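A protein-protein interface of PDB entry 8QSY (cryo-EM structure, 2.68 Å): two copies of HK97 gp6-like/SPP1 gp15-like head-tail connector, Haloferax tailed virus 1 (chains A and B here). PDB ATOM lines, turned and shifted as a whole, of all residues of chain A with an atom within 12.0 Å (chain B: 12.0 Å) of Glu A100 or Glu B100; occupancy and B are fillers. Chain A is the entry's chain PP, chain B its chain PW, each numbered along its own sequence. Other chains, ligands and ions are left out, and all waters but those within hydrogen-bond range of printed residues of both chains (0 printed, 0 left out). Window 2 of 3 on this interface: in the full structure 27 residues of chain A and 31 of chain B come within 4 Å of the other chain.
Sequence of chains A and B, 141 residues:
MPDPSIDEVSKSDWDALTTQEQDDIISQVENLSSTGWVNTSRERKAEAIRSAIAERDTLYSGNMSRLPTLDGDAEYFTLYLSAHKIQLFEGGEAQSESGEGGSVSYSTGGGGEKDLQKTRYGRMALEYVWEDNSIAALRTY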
ATOM      1  N   SER A  96      20.702   2.635 -16.884  1.00  0.00           N
ATOM      2  CA  SER A  96      19.596   3.271 -16.182  1.00  0.00           C
ATOM      3  C   SER A  96      18.689   3.987 -17.175  1.00  0.00           C
ATOM      4  O   SER A  96      19.149   4.478 -18.204  1.00  0.00           O
ATOM      5  CB  SER A  96      20.098   4.183 -15.096  1.00  0.00           C
ATOM      6  OG  SER A  96      19.026   4.858 -14.460  1.00  0.00           O
ATOM      7  N   GLU A  97      17.387   4.000 -16.867  1.00  0.00           N
ATOM      8  CA  GLU A  97      16.349   4.631 -17.666  1.00  0.00           C
ATOM      9  C   GLU A  97      15.470   5.457 -16.727  1.00  0.00           C
ATOM     10  O   GLU A  97      15.213   5.049 -15.598  1.00  0.00           O
ATOM     11  CB  GLU A  97      15.520   3.563 -18.383  1.00  0.00           C
ATOM     12  CG  GLU A  97      16.323   2.661 -19.304  1.00  0.00           C
ATOM     13  CD  GLU A  97      15.471   1.590 -19.970  1.00  0.00           C
ATOM     14  OE1 GLU A  97      15.106   0.603 -19.291  1.00  0.00           O
ATOM     15  OE2 GLU A  97      15.195   1.734 -21.177  1.00  0.00           O
ATOM     16  N   SER A  98      15.019   6.631 -17.184  1.00  0.00           N
ATOM     17  CA  SER A  98      14.244   7.546 -16.349  1.00  0.00           C
ATOM     18  C   SER A  98      13.289   8.369 -17.220  1.00  0.00           C
ATOM     19  O   SER A  98      13.637   8.725 -18.347  1.00  0.00           O
ATOM     20  CB  SER A  98      15.183   8.443 -15.583  1.00  0.00           C
ATOM     21  OG  SER A  98      14.471   9.331 -14.736  1.00  0.00           O
ATOM     22  N   GLY A  99      12.103   8.696 -16.684  1.00  0.00           N
ATOM     23  CA  GLY A  99      11.094   9.467 -17.399  1.00  0.00           C
ATOM     24  C   GLY A  99       9.867   9.760 -16.538  1.00  0.00           C
ATOM     25  O   GLY A  99       9.899   9.607 -15.315  1.00  0.00           O
ATOM     26  N   GLU A 100       8.758  10.125 -17.195  1.00  0.00           N
ATOM     27  CA  GLU A 100       7.501  10.413 -16.514  1.00  0.00           C
ATOM     28  C   GLU A 100       6.943   9.164 -15.817  1.00  0.00           C
ATOM     29  O   GLU A 100       6.365   9.262 -14.732  1.00  0.00           O
ATOM     30  CB  GLU A 100       6.494  11.012 -17.495  1.00  0.00           C
ATOM     31  CG  GLU A 100       6.900  12.381 -18.029  1.00  0.00           C
ATOM     32  CD  GLU A 100       7.094  13.489 -17.002  1.00  0.00           C
ATOM     33  OE1 GLU A 100       6.264  13.592 -16.070  1.00  0.00           O
ATOM     34  OE2 GLU A 100       8.070  14.259 -17.139  1.00  0.00           O
ATOM     35  N   GLY A 101       7.154   7.979 -16.412  1.00  0.00           N
ATOM     36  CA  GLY A 101       6.625   6.719 -15.897  1.00  0.00           C
ATOM     37  C   GLY A 101       7.428   6.117 -14.736  1.00  0.00           C
ATOM     38  O   GLY A 101       7.124   5.003 -14.303  1.00  0.00           O
ATOM     39  N   GLY A 102       8.452   6.837 -14.246  1.00  0.00           N
ATOM     40  CA  GLY A 102       9.332   6.399 -13.167  1.00  0.00           C
ATOM     41  C   GLY A 102      10.795   6.296 -13.602  1.00  0.00           C
ATOM     42  O   GLY A 102      11.176   6.817 -14.649  1.00  0.00           O
ATOM     43  N   SER A 103      11.621   5.639 -12.773  1.00  0.00           N
ATOM     44  CA  SER A 103      13.034   5.420 -13.067  1.00  0.00           C
ATOM     45  C   SER A 103      13.464   4.018 -12.637  1.00  0.00           C
ATOM     46  O   SER A 103      12.942   3.460 -11.677  1.00  0.00           O
ATOM     47  CB  SER A 103      13.917   6.442 -12.403  1.00  0.00           C
ATOM     48  OG  SER A 103      13.534   7.762 -12.745  1.00  0.00           O
ATOM     49  N   VAL A 104      14.447   3.458 -13.347  1.00  0.00           N
ATOM     50  CA  VAL A 104      15.008   2.155 -13.022  1.00  0.00           C
ATOM     51  C   VAL A 104      16.517   2.175 -13.270  1.00  0.00           C
ATOM     52  O   VAL A 104      17.018   2.854 -14.168  1.00  0.00           O
ATOM     53  CB  VAL A 104      14.291   1.018 -13.782  1.00  0.00           C
ATOM     54  CG1 VAL A 104      14.368   1.199 -15.288  1.00  0.00           C
ATOM     55  CG2 VAL A 104      14.805  -0.364 -13.402  1.00  0.00           C
ATOM     56  N   SER B  96      17.615  -0.781  -8.650  1.00  0.00           N
ATOM     57  CA  SER B  96      16.738   0.166  -7.974  1.00  0.00           C
ATOM     58  C   SER B  96      15.556   0.520  -8.873  1.00  0.00           C
ATOM     59  O   SER B  96      15.677   0.534 -10.094  1.00  0.00           O
ATOM     60  CB  SER B  96      17.507   1.382  -7.529  1.00  0.00           C
ATOM     61  OG  SER B  96      16.646   2.349  -6.958  1.00  0.00           O
ATOM     62  N   GLU B  97      14.403   0.781  -8.247  1.00  0.00           N
ATOM     63  CA  GLU B  97      13.159   1.121  -8.920  1.00  0.00           C
ATOM     64  C   GLU B  97      12.541   2.328  -8.213  1.00  0.00           C
ATOM     65  O   GLU B  97      12.486   2.369  -6.984  1.00  0.00           O
ATOM     66  CB  GLU B  97      12.189  -0.058  -8.856  1.00  0.00           C
ATOM     67  CG  GLU B  97      12.688  -1.320  -9.541  1.00  0.00           C
ATOM     68  CD  GLU B  97      11.780  -2.522  -9.319  1.00  0.00           C
ATOM     69  OE1 GLU B  97      11.608  -2.937  -8.152  1.00  0.00           O
ATOM     70  OE2 GLU B  97      11.242  -3.046 -10.317  1.00  0.00           O
ATOM     71  N   SER B  98      12.076   3.310  -8.994  1.00  0.00           N
ATOM     72  CA  SER B  98      11.487   4.525  -8.451  1.00  0.00           C
ATOM     73  C   SER B  98      10.234   4.888  -9.247  1.00  0.00           C
ATOM     74  O   SER B  98      10.223   4.767 -10.468  1.00  0.00           O
ATOM     75  CB  SER B  98      12.508   5.636  -8.437  1.00  0.00           C
ATOM     76  OG  SER B  98      11.946   6.836  -7.935  1.00  0.00           O
ATOM     77  N   GLY B  99       9.181   5.314  -8.540  1.00  0.00           N
ATOM     78  CA  GLY B  99       7.869   5.536  -9.127  1.00  0.00           C
ATOM     79  C   GLY B  99       7.265   6.860  -8.672  1.00  0.00           C
ATOM     80  O   GLY B  99       7.956   7.876  -8.639  1.00  0.00           O
ATOM     81  N   GLU B 100       5.977   6.828  -8.310  1.00  0.00           N
ATOM     82  CA  GLU B 100       5.250   8.010  -7.868  1.00  0.00           C
ATOM     83  C   GLU B 100       5.599   8.325  -6.410  1.00  0.00           C
ATOM     84  O   GLU B 100       4.798   8.104  -5.502  1.00  0.00           O
ATOM     85  CB  GLU B 100       3.752   7.825  -8.128  1.00  0.00           C
ATOM     86  CG  GLU B 100       3.418   7.643  -9.602  1.00  0.00           C
ATOM     87  CD  GLU B 100       4.026   8.673 -10.543  1.00  0.00           C
ATOM     88  OE1 GLU B 100       3.894   9.886 -10.260  1.00  0.00           O
ATOM     89  OE2 GLU B 100       4.636   8.265 -11.556  1.00  0.00           O
ATOM     90  N   GLY B 101       6.810   8.859  -6.198  1.00  0.00           N
ATOM     91  CA  GLY B 101       7.340   9.155  -4.870  1.00  0.00           C
ATOM     92  C   GLY B 101       7.949   7.937  -4.161  1.00  0.00           C
ATOM     93  O   GLY B 101       8.913   8.076  -3.402  1.00  0.00           O
ATOM     94  N   GLY B 102       7.376   6.747  -4.386  1.00  0.00           N
ATOM     95  CA  GLY B 102       7.870   5.496  -3.824  1.00  0.00           C
ATOM     96  C   GLY B 102       9.176   5.060  -4.485  1.00  0.00           C
ATOM     97  O   GLY B 102       9.354   5.238  -5.689  1.00  0.00           O
ATOM     98  N   SER B 103      10.087   4.483  -3.691  1.00  0.00           N
ATOM     99  CA  SER B 103      11.405   4.099  -4.181  1.00  0.00           C
ATOM    100  C   SER B 103      11.968   2.917  -3.393  1.00  0.00           C
ATOM    101  O   SER B 103      11.733   2.794  -2.196  1.00  0.00           O
ATOM    102  CB  SER B 103      12.344   5.275  -4.137  1.00  0.00           C
ATOM    103  OG  SER B 103      13.642   4.912  -4.579  1.00  0.00           O
ATOM    104  N   VAL B 104      12.741   2.058  -4.075  1.00  0.00           N
ATOM    105  CA  VAL B 104      13.425   0.937  -3.444  1.00  0.00           C
ATOM    106  C   VAL B 104      14.775   0.692  -4.126  1.00  0.00           C
ATOM    107  O   VAL B 104      14.957   0.946  -5.316  1.00  0.00           O
ATOM    108  CB  VAL B 104      12.541  -0.328  -3.403  1.00  0.00           C
ATOM    109  CG1 VAL B 104      12.157  -0.794  -4.795  1.00  0.00           C
ATOM    110  CG2 VAL B 104      13.185  -1.481  -2.636  1.00  0.00           C
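Of chain B, only Glu B100 (3.8 Å) comes within 4 Å of Glu A100.
No residue of chain B comes within 4 Å of Gly A101.
Gly A102 touches one residue of chain B.
Of the printed residues of chain B, Ser A103 touches Glu B97 and Ser B98.
Of the printed residues of chain B, Val A104 touches Ser B96.
Printed residues of chain A within 4 Å of Ser B96: Val A104 (3.4 Å).
Of the printed residues of chain A, Glu B97 touches Ser A103 (3.6 Å).
No residue of chain A comes within 4 Å of Gly B99.
Glu B100 touches one residue of chain A.
No residue of chain A comes within 4 Å of Gly B101.
Val B104 touches none of the printed residues of chain A.
The nearest residue of chain B that does not touch Glu A100 is Gly B99 (6.4 Å).
OG of Ser A96 is in hydrogen-bond range of O of Val A104 (2.9 Å).
O of Glu A97 is in hydrogen-bond range of N of Val A104, at 2.9 Å.
The side-chain hydroxyl (OG) of Ser A103 sits at hydrogen-bond distance from the side-chain hydroxyl (OG) of Ser A98 (2.7 Å).
The backbone carbonyl oxygen of Val B104 lies within hydrogen-bond range of the side-chain hydroxyl of Ser B96, 2.7 Å away.
O of Glu B97 sits at hydrogen-bond distance from N of Val B104.
Of the 9 printed residues of chain A, 4 touch a printed residue of chain B.
Printed residues of chain A that touch a printed residue of chain B: Glu A100, Gly A102, Ser A103 and Val A104.
Glu B100 touches its own counterpart, Glu A100.
Ser A103 touches Glu B97, but with the chains exchanged Glu A97 does not touch Ser B103 (11.1 Å).
Ser A103 touches Ser B98, but with the chains exchanged Ser A98 does not touch Ser B103 (11.1 Å).
Val A104 touches Ser B96, but with the chains exchanged Ser A96 does not touch Val B104 (10.7 Å).
9 positions are printed for both chains.
Of the 5 pairs that touch across the chains among the printed residues, 1 has its exchanged pair printed and touching as well.
The backbone carbonyl oxygen (O) of Ser A103 sits at hydrogen-bond distance from the backbone NH (N) of Ser B98 (2.8 Å).
Glu A100 touches Glu B100 (O to OE2, 3.8 Å).
O of Ser B98 touches CA of Gly A102, 3.3 Å away.
CA of Glu B97 touches O of Ser A103, at 3.6 Å.
Val A104 touches Ser B96 (CA to O, 3.4 Å).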
